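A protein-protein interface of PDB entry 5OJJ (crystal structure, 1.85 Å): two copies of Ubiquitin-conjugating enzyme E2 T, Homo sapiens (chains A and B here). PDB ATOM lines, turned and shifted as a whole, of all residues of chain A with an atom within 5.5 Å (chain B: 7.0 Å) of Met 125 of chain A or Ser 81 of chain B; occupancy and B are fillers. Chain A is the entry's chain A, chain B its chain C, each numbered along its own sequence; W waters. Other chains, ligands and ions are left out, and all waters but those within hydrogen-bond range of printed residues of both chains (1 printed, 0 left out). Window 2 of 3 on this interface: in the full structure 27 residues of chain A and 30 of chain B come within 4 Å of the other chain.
Of the printed residues of chain B, Pro 123 of chain A touches Trp 146 and His 150.
Asp 127 of chain A touches none of the printed residues of chain B.
Of the printed residues of chain A, Pro 73 of chain B touches Arg 84 (3.8 Å) and Leu 124 (3.6 Å).
Ile 74 of chain B touches none of the printed residues of chain A.
Of the printed residues of chain A, Ser 81 of chain B touches Asp 80, Ala 82, Arg 84 and Met 125.
The nearest residue of chain B that does not touch Met 125 of chain A is Trp 146 of chain B (4.2 Å).
The nearest printed residue of chain A that does not touch Ser 81 of chain B is Ser 81 of chain A (4.1 Å).
The nearest printed residue of chain B that does not touch Ala 82 of chain A is Gly 83 of chain B (5.6 Å).
Ser 81 of chain B touches Ala 82 of chain A (O to CB, 3.99 Å).
Ala 82 of chain A touches Ala 82 of chain B.
NH1 of Arg 84 of chain A touches N of Pro 73 of chain B, at 3.8 Å.
Arg 84 of chain A touches Gly 83 of chain B (NH2 to N, 3.9 Å).
O of Pro 123 of chain A touches CZ2 of Trp 146 of chain B, 3.5 Å away.
CD2 of Leu 124 of chain A touches CG of Pro 73 of chain B, at 3.6 Å.
O of Leu 124 of chain A touches CH2 of Trp 146 of chain B, 3.3 Å away.
CD2 of Leu 124 of chain A touches CE1 of His 150 of chain B (3.4 Å).
Met 125 of chain A touches Ser 81 of chain B.
Water W1 lies within hydrogen-bond range of OG of Ser 81 of chain B (2.8 Å) and O of Leu 124 of chain A (3.0 Å).
NH2 of Arg 84 of chain A is in hydrogen-bond range of O of Ser 81 of chain B, at 2.8 Å.
The backbone carbonyl oxygen of Pro 123 of chain A is in hydrogen-bond range of a ring nitrogen (NE2) of His 150 of chain B (2.9 Å).
The side-chain carboxylate (OD2) of Asp 80 of chain A lies close to the backbone carbonyl oxygen (O) of Ser 81 of chain B, at 3.3 Å.
Printed residues of chain B that touch a printed residue of chain A: Pro 73, Ser 81, Ala 82, Gly 83, Trp 146 and His 150.
Hydrophobic or aromatic side chains of chain A that line the printed part of chain B: Ala 82, Pro 123, Leu 124 and Met 125.
Along chain A the printed residues that touch a printed residue of chain B span positions 80 to 125.
The backbone NH (N) of Leu 124 of chain A sits at hydrogen-bond distance from the backbone carbonyl oxygen (O) of Pro 77 of chain A (3.0 Å).
The side-chain carboxylate (OD1) of Asp 80 of chain A is in hydrogen-bond range of the backbone NH (N) of Ala 82 of chain A, 3.0 Å away.
The guanidinium group (NE) of Arg 84 of chain A is in salt-bridge range of the side-chain carboxylate (OD2) of Asp 80 of chain A, at 2.9 Å.
OD1 of Asp 80 of chain B sits at hydrogen-bond distance from N of Ala 82 of chain B, 3.1 Å away.
N of Gly 83 of chain B is in hydrogen-bond range of OD1 of Asp 80 of chain B (3.3 Å).
The backbone NH of Ser 81 of chain B is in hydrogen-bond range of the side-chain sulfur of Met 125 of chain B.
Asp 80 of chain A touches Ser 81 of chain B, but with the chains exchanged Ser 81 of chain A does not touch Asp 80 of chain B (7.4 Å).
Ala 82 of chain B touches its own counterpart, Ala 82 of chain A.
Arg 84 of chain A touches Ser 81 of chain B, but with the chains exchanged Ser 81 of chain A does not touch Arg 84 of chain B (8.3 Å).
Met 125 of chain A touches Ser 81 of chain B, but with the chains exchanged Ser 81 of chain A does not touch Met 125 of chain B (7.5 Å).
Of the 12 pairs that touch across the chains among the printed residues, 1 has its exchanged pair printed and touching as well.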
ATOM      1  N   HIS A  76       5.272 -12.655   0.877  1.00  0.00           N
ATOM      2  CA  HIS A  76       4.682 -11.316   0.650  1.00  0.00           C
ATOM      3  C   HIS A  76       3.155 -11.452   0.735  1.00  0.00           C
ATOM      4  O   HIS A  76       2.571 -12.408   0.183  1.00  0.00           O
ATOM      5  CB  HIS A  76       5.166 -10.808  -0.733  1.00  0.00           C
ATOM      6  CG  HIS A  76       4.862  -9.371  -1.045  1.00  0.00           C
ATOM      7  ND1 HIS A  76       3.594  -8.924  -1.342  1.00  0.00           N
ATOM      8  CD2 HIS A  76       5.680  -8.303  -1.224  1.00  0.00           C
ATOM      9  CE1 HIS A  76       3.629  -7.638  -1.640  1.00  0.00           C
ATOM     10  NE2 HIS A  76       4.883  -7.232  -1.568  1.00  0.00           N
ATOM     11  N   PRO A  77       2.475 -10.529   1.443  1.00  0.00           N
ATOM     12  CA  PRO A  77       1.028 -10.724   1.646  1.00  0.00           C
ATOM     13  C   PRO A  77       0.129 -10.684   0.391  1.00  0.00           C
ATOM     14  O   PRO A  77      -0.964 -11.242   0.417  1.00  0.00           O
ATOM     15  CB  PRO A  77       0.649  -9.576   2.591  1.00  0.00           C
ATOM     16  CG  PRO A  77       1.680  -8.550   2.396  1.00  0.00           C
ATOM     17  CD  PRO A  77       2.952  -9.272   2.056  1.00  0.00           C
ATOM     18  N   ILE A  79       1.071 -11.822  -2.772  1.00  0.00           N
ATOM     19  CA  ILE A  79       1.544 -12.809  -3.770  1.00  0.00           C
ATOM     20  C   ILE A  79       1.342 -14.218  -3.178  1.00  0.00           C
ATOM     21  O   ILE A  79       1.776 -14.462  -2.053  1.00  0.00           O
ATOM     22  CB  ILE A  79       3.033 -12.553  -4.129  1.00  0.00           C
ATOM     23  CG1 ILE A  79       3.240 -11.090  -4.607  1.00  0.00           C
ATOM     24  CG2 ILE A  79       3.521 -13.518  -5.204  1.00  0.00           C
ATOM     25  CD1 ILE A  79       4.666 -10.612  -4.575  1.00  0.00           C
ATOM     26  N   ASP A  80       0.688 -15.134  -3.902  1.00  0.00           N
ATOM     27  CA  ASP A  80       0.460 -16.498  -3.371  1.00  0.00           C
ATOM     28  C   ASP A  80       1.462 -17.555  -3.883  1.00  0.00           C
ATOM     29  O   ASP A  80       2.429 -17.234  -4.603  1.00  0.00           O
ATOM     30  CB  ASP A  80      -1.026 -16.894  -3.520  1.00  0.00           C
ATOM     31  CG  ASP A  80      -1.478 -17.087  -4.961  1.00  0.00           C
ATOM     32  OD1 ASP A  80      -0.661 -17.385  -5.867  1.00  0.00           O
ATOM     33  OD2 ASP A  80      -2.699 -16.959  -5.190  1.00  0.00           O
ATOM     34  N   SER A  81       1.228 -18.805  -3.471  1.00  0.00           N
ATOM     35  CA  SER A  81       2.001 -19.985  -3.895  1.00  0.00           C
ATOM     36  C   SER A  81       1.956 -20.301  -5.391  1.00  0.00           C
ATOM     37  O   SER A  81       2.909 -20.863  -5.906  1.00  0.00           O
ATOM     38  CB  SER A  81       1.520 -21.224  -3.108  1.00  0.00           C
ATOM     39  OG  SER A  81       1.575 -20.968  -1.735  1.00  0.00           O
ATOM     40  N   ALA A  82       0.879 -19.937  -6.088  1.00  0.00           N
ATOM     41  CA  ALA A  82       0.837 -20.006  -7.560  1.00  0.00           C
ATOM     42  C   ALA A  82       1.556 -18.829  -8.242  1.00  0.00           C
ATOM     43  O   ALA A  82       1.631 -18.751  -9.475  1.00  0.00           O
ATOM     44  CB  ALA A  82      -0.595 -20.068  -8.045  1.00  0.00           C
ATOM     45  N   ARG A  84       0.465 -15.715  -8.089  1.00  0.00           N
ATOM     46  CA  ARG A  84      -0.518 -14.726  -8.497  1.00  0.00           C
ATOM     47  C   ARG A  84      -0.321 -13.459  -7.674  1.00  0.00           C
ATOM     48  O   ARG A  84       0.080 -13.552  -6.493  1.00  0.00           O
ATOM     49  CB  ARG A  84      -1.948 -15.231  -8.308  1.00  0.00           C
ATOM     50  CG  ARG A  84      -2.292 -16.424  -9.181  1.00  0.00           C
ATOM     51  CD  ARG A  84      -3.711 -16.932  -8.986  1.00  0.00           C
ATOM     52  NE  ARG A  84      -3.898 -17.620  -7.707  1.00  0.00           N
ATOM     53  CZ  ARG A  84      -4.932 -18.396  -7.373  1.00  0.00           C
ATOM     54  NH1 ARG A  84      -5.924 -18.642  -8.224  1.00  0.00           N
ATOM     55  NH2 ARG A  84      -4.968 -18.956  -6.172  1.00  0.00           N
ATOM     56  N   PRO A 123      -5.130  -9.161   0.748  1.00  0.00           N
ATOM     57  CA  PRO A 123      -4.426 -10.442   0.969  1.00  0.00           C
ATOM     58  C   PRO A 123      -4.675 -11.542  -0.077  1.00  0.00           C
ATOM     59  O   PRO A 123      -5.821 -11.769  -0.481  1.00  0.00           O
ATOM     60  CB  PRO A 123      -4.983 -10.898   2.325  1.00  0.00           C
ATOM     61  CG  PRO A 123      -6.379 -10.352   2.336  1.00  0.00           C
ATOM     62  CD  PRO A 123      -6.269  -9.002   1.675  1.00  0.00           C
ATOM     63  N   LEU A 124      -3.605 -12.220  -0.496  1.00  0.00           N
ATOM     64  CA  LEU A 124      -3.711 -13.528  -1.162  1.00  0.00           C
ATOM     65  C   LEU A 124      -3.176 -14.704  -0.319  1.00  0.00           C
ATOM     66  O   LEU A 124      -3.370 -15.853  -0.700  1.00  0.00           O
ATOM     67  CB  LEU A 124      -3.006 -13.512  -2.522  1.00  0.00           C
ATOM     68  CG  LEU A 124      -3.632 -12.703  -3.661  1.00  0.00           C
ATOM     69  CD1 LEU A 124      -2.753 -12.813  -4.902  1.00  0.00           C
ATOM     70  CD2 LEU A 124      -5.053 -13.169  -3.952  1.00  0.00           C
ATOM     71  N   MET A 125      -2.474 -14.423   0.786  1.00  0.00           N
ATOM     72  CA  MET A 125      -2.041 -15.444   1.724  1.00  0.00           C
ATOM     73  C   MET A 125      -2.426 -14.970   3.137  1.00  0.00           C
ATOM     74  O   MET A 125      -1.857 -14.007   3.641  1.00  0.00           O
ATOM     75  CB  MET A 125      -0.535 -15.693   1.608  1.00  0.00           C
ATOM     76  CG  MET A 125      -0.068 -16.209   0.247  1.00  0.00           C
ATOM     77  SD  MET A 125      -0.566 -17.910  -0.105  1.00  0.00           S
ATOM     78  CE  MET A 125       0.799 -18.780   0.665  1.00  0.00           C
ATOM     79  N   ALA A 126      -3.384 -15.660   3.751  1.00  0.00           N
ATOM     80  CA  ALA A 126      -4.005 -15.206   5.008  1.00  0.00           C
ATOM     81  C   ALA A 126      -3.027 -15.071   6.178  1.00  0.00           C
ATOM     82  O   ALA A 126      -2.981 -14.007   6.807  1.00  0.00           O
ATOM     83  CB  ALA A 126      -5.173 -16.117   5.378  1.00  0.00           C
ATOM     84  N   ASP A 127      -2.227 -16.105   6.443  1.00  0.00           N
ATOM     85  CA  ASP A 127      -1.230 -16.061   7.537  1.00  0.00           C
ATOM     86  C   ASP A 127      -0.186 -14.955   7.350  1.00  0.00           C
ATOM     87  O   ASP A 127       0.244 -14.315   8.325  1.00  0.00           O
ATOM     88  CB  ASP A 127      -0.479 -17.398   7.687  1.00  0.00           C
ATOM     89  CG  ASP A 127      -1.297 -18.484   8.392  1.00  0.00           C
ATOM     90  OD1 ASP A 127      -2.492 -18.280   8.724  1.00  0.00           O
ATOM     91  OD2 ASP A 127      -0.718 -19.577   8.590  1.00  0.00           O
ATOM     92  N   ILE A 128       0.232 -14.747   6.099  1.00  0.00           N
ATOM     93  CA  ILE A 128       1.244 -13.741   5.795  1.00  0.00           C
ATOM     94  C   ILE A 128       0.660 -12.335   6.008  1.00  0.00           C
ATOM     95  O   ILE A 128       1.321 -11.491   6.621  1.00  0.00           O
ATOM     96  CB  ILE A 128       1.865 -13.927   4.396  1.00  0.00           C
ATOM     97  CG1 ILE A 128       2.549 -15.298   4.298  1.00  0.00           C
ATOM     98  CG2 ILE A 128       2.904 -12.844   4.111  1.00  0.00           C
ATOM     99  CD1 ILE A 128       3.139 -15.633   2.951  1.00  0.00           C
ATOM    100  N   SER A 129      -0.562 -12.093   5.539  1.00  0.00           N
ATOM    101  CA  SER A 129      -1.233 -10.799   5.747  1.00  0.00           C
ATOM    102  C   SER A 129      -1.444 -10.440   7.234  1.00  0.00           C
ATOM    103  O   SER A 129      -1.140  -9.320   7.679  1.00  0.00           O
ATOM    104  CB  SER A 129      -2.578 -10.797   5.051  1.00  0.00           C
ATOM    105  OG  SER A 129      -3.133  -9.493   5.071  1.00  0.00           O
ATOM    106  N   SER A 130      -1.995 -11.396   7.982  1.00  0.00           N
ATOM    107  CA  SER A 130      -2.140 -11.250   9.435  1.00  0.00           C
ATOM    108  C   SER A 130      -0.829 -10.864  10.120  1.00  0.00           C
ATOM    109  O   SER A 130      -0.771  -9.892  10.881  1.00  0.00           O
ATOM    110  CB  SER A 130      -2.701 -12.536  10.028  1.00  0.00           C
ATOM    111  OG  SER A 130      -4.061 -12.635   9.636  1.00  0.00           O
ATOM    112  N   PRO B  73      -8.571 -16.037  -7.606  1.00  0.00           N
ATOM    113  CA  PRO B  73      -8.508 -16.438  -6.201  1.00  0.00           C
ATOM    114  C   PRO B  73      -9.875 -16.552  -5.551  1.00  0.00           C
ATOM    115  O   PRO B  73     -10.783 -15.804  -5.909  1.00  0.00           O
ATOM    116  CB  PRO B  73      -7.694 -15.312  -5.522  1.00  0.00           C
ATOM    117  CG  PRO B  73      -6.968 -14.638  -6.614  1.00  0.00           C
ATOM    118  CD  PRO B  73      -7.783 -14.814  -7.870  1.00  0.00           C
ATOM    119  N   ILE B  74     -10.022 -17.499  -4.618  1.00  0.00           N
ATOM    120  CA  ILE B  74     -11.307 -17.755  -3.948  1.00  0.00           C
ATOM    121  C   ILE B  74     -10.991 -18.343  -2.567  1.00  0.00           C
ATOM    122  O   ILE B  74     -10.056 -19.163  -2.444  1.00  0.00           O
ATOM    123  CB  ILE B  74     -12.265 -18.671  -4.793  1.00  0.00           C
ATOM    124  CG1 ILE B  74     -13.642 -18.818  -4.123  1.00  0.00           C
ATOM    125  CG2 ILE B  74     -11.645 -20.045  -5.076  1.00  0.00           C
ATOM    126  CD1 ILE B  74     -14.681 -19.565  -4.962  1.00  0.00           C
ATOM    127  N   ILE B  79     -10.682 -25.494  -1.916  1.00  0.00           N
ATOM    128  CA  ILE B  79      -9.984 -24.867  -3.038  1.00  0.00           C
ATOM    129  C   ILE B  79      -8.732 -24.170  -2.516  1.00  0.00           C
ATOM    130  O   ILE B  79      -8.835 -23.272  -1.670  1.00  0.00           O
ATOM    131  CB  ILE B  79     -10.893 -23.877  -3.779  1.00  0.00           C
ATOM    132  CG1 ILE B  79     -12.214 -24.568  -4.184  1.00  0.00           C
ATOM    133  CG2 ILE B  79     -10.196 -23.326  -5.022  1.00  0.00           C
ATOM    134  CD1 ILE B  79     -13.334 -23.638  -4.588  1.00  0.00           C
ATOM    135  N   ASP B  80      -7.561 -24.562  -3.015  1.00  0.00           N
ATOM    136  CA  ASP B  80      -6.305 -24.102  -2.380  1.00  0.00           C
ATOM    137  C   ASP B  80      -5.651 -22.860  -3.000  1.00  0.00           C
ATOM    138  O   ASP B  80      -6.128 -22.313  -4.008  1.00  0.00           O
ATOM    139  CB  ASP B  80      -5.329 -25.277  -2.135  1.00  0.00           C
ATOM    140  CG  ASP B  80      -4.720 -25.851  -3.392  1.00  0.00           C
ATOM    141  OD1 ASP B  80      -4.624 -25.173  -4.439  1.00  0.00           O
ATOM    142  OD2 ASP B  80      -4.282 -27.030  -3.324  1.00  0.00           O
ATOM    143  N   SER B  81      -4.547 -22.420  -2.376  1.00  0.00           N
ATOM    144  CA  SER B  81      -3.751 -21.259  -2.843  1.00  0.00           C
ATOM    145  C   SER B  81      -3.272 -21.286  -4.260  1.00  0.00           C
ATOM    146  O   SER B  81      -2.882 -20.235  -4.776  1.00  0.00           O
ATOM    147  CB  SER B  81      -2.497 -21.096  -1.964  1.00  0.00           C
ATOM    148  OG  SER B  81      -2.922 -20.840  -0.663  1.00  0.00           O
ATOM    149  N   ALA B  82      -3.252 -22.477  -4.872  1.00  0.00           N
ATOM    150  CA  ALA B  82      -2.895 -22.655  -6.260  1.00  0.00           C
ATOM    151  C   ALA B  82      -4.105 -22.876  -7.165  1.00  0.00           C
ATOM    152  O   ALA B  82      -3.950 -23.125  -8.361  1.00  0.00           O
ATOM    153  CB  ALA B  82      -1.946 -23.837  -6.392  1.00  0.00           C
ATOM    154  N   GLY B  83      -5.297 -22.821  -6.581  1.00  0.00           N
ATOM    155  CA  GLY B  83      -6.552 -23.020  -7.310  1.00  0.00           C
ATOM    156  C   GLY B  83      -6.992 -24.463  -7.533  1.00  0.00           C
ATOM    157  O   GLY B  83      -7.975 -24.704  -8.239  1.00  0.00           O
ATOM    158  N   ARG B  84      -6.271 -25.422  -6.959  1.00  0.00           N
ATOM    159  CA  ARG B  84      -6.670 -26.841  -7.049  1.00  0.00           C
ATOM    160  C   ARG B  84      -7.994 -27.091  -6.292  1.00  0.00           C
ATOM    161  O   ARG B  84      -8.262 -26.447  -5.283  1.00  0.00           O
ATOM    162  CB  ARG B  84      -5.535 -27.740  -6.534  1.00  0.00           C
ATOM    163  CG  ARG B  84      -4.275 -27.572  -7.386  1.00  0.00           C
ATOM    164  CD  ARG B  84      -3.158 -28.532  -7.024  1.00  0.00           C
ATOM    165  NE  ARG B  84      -2.826 -28.462  -5.610  1.00  0.00           N
ATOM    166  CZ  ARG B  84      -1.770 -29.043  -5.031  1.00  0.00           C
ATOM    167  NH1 ARG B  84      -0.890 -29.750  -5.754  1.00  0.00           N
ATOM    168  NH2 ARG B  84      -1.605 -28.907  -3.704  1.00  0.00           N
ATOM    169  N   LEU B 124      -8.527 -28.979   1.514  1.00  0.00           N
ATOM    170  CA  LEU B 124      -7.253 -28.646   0.866  1.00  0.00           C
ATOM    171  C   LEU B 124      -6.578 -27.445   1.510  1.00  0.00           C
ATOM    172  O   LEU B 124      -5.413 -27.171   1.212  1.00  0.00           O
ATOM    173  CB  LEU B 124      -7.416 -28.375  -0.644  1.00  0.00           C
ATOM    174  CG  LEU B 124      -7.450 -29.559  -1.597  1.00  0.00           C
ATOM    175  CD1 LEU B 124      -7.671 -29.054  -3.021  1.00  0.00           C
ATOM    176  CD2 LEU B 124      -6.202 -30.419  -1.530  1.00  0.00           C
ATOM    177  N   MET B 125      -7.316 -26.717   2.351  1.00  0.00           N
ATOM    178  CA  MET B 125      -6.827 -25.494   3.006  1.00  0.00           C
ATOM    179  C   MET B 125      -7.203 -25.635   4.472  1.00  0.00           C
ATOM    180  O   MET B 125      -8.349 -25.387   4.850  1.00  0.00           O
ATOM    181  CB  MET B 125      -7.447 -24.230   2.371  1.00  0.00           C
ATOM    182  CG  MET B 125      -6.805 -23.809   1.051  1.00  0.00           C
ATOM    183  SD  MET B 125      -5.015 -23.491   0.985  1.00  0.00           S
ATOM    184  CE  MET B 125      -5.033 -21.807   1.616  1.00  0.00           C
ATOM    185  N   ILE B 128      -8.529 -22.528   6.532  1.00  0.00           N
ATOM    186  CA  ILE B 128      -9.884 -22.127   6.125  1.00  0.00           C
ATOM    187  C   ILE B 128     -10.906 -23.153   6.626  1.00  0.00           C
ATOM    188  O   ILE B 128     -11.993 -22.783   7.051  1.00  0.00           O
ATOM    189  CB  ILE B 128     -10.013 -21.913   4.589  1.00  0.00           C
ATOM    190  CG1 ILE B 128      -8.976 -20.885   4.104  1.00  0.00           C
ATOM    191  CG2 ILE B 128     -11.433 -21.443   4.246  1.00  0.00           C
ATOM    192  CD1 ILE B 128      -8.972 -20.563   2.619  1.00  0.00           C
ATOM    193  N   TRP B 146     -12.685 -11.368   0.228  1.00  0.00           N
ATOM    194  CA  TRP B 146     -11.909 -11.934  -0.901  1.00  0.00           C
ATOM    195  C   TRP B 146     -12.690 -11.852  -2.223  1.00  0.00           C
ATOM    196  O   TRP B 146     -12.123 -11.592  -3.277  1.00  0.00           O
ATOM    197  CB  TRP B 146     -11.439 -13.382  -0.622  1.00  0.00           C
ATOM    198  CG  TRP B 146     -10.229 -13.477   0.279  1.00  0.00           C
ATOM    199  CD1 TRP B 146     -10.066 -12.864   1.497  1.00  0.00           C
ATOM    200  CD2 TRP B 146      -9.022 -14.224   0.052  1.00  0.00           C
ATOM    201  NE1 TRP B 146      -8.839 -13.168   2.022  1.00  0.00           N
ATOM    202  CE2 TRP B 146      -8.177 -13.998   1.162  1.00  0.00           C
ATOM    203  CE3 TRP B 146      -8.567 -15.050  -0.986  1.00  0.00           C
ATOM    204  CZ2 TRP B 146      -6.919 -14.588   1.279  1.00  0.00           C
ATOM    205  CZ3 TRP B 146      -7.315 -15.608  -0.879  1.00  0.00           C
ATOM    206  CH2 TRP B 146      -6.509 -15.392   0.250  1.00  0.00           C
ATOM    207  N   HIS B 150     -10.892  -9.717  -5.220  1.00  0.00           N
ATOM    208  CA  HIS B 150     -10.294 -10.481  -6.329  1.00  0.00           C
ATOM    209  C   HIS B 150     -11.234 -10.925  -7.452  1.00  0.00           C
ATOM    210  O   HIS B 150     -10.776 -11.242  -8.552  1.00  0.00           O
ATOM    211  CB  HIS B 150      -9.619 -11.732  -5.766  1.00  0.00           C
ATOM    212  CG  HIS B 150      -8.754 -11.464  -4.583  1.00  0.00           C
ATOM    213  ND1 HIS B 150      -7.760 -10.514  -4.596  1.00  0.00           N
ATOM    214  CD2 HIS B 150      -8.736 -12.015  -3.350  1.00  0.00           C
ATOM    215  CE1 HIS B 150      -7.159 -10.494  -3.419  1.00  0.00           C
ATOM    216  NE2 HIS B 150      -7.741 -11.391  -2.643  1.00  0.00           N
HETATM  217  O   HOH W   1      -4.385 -18.576  -0.102  1.00  0.00           O
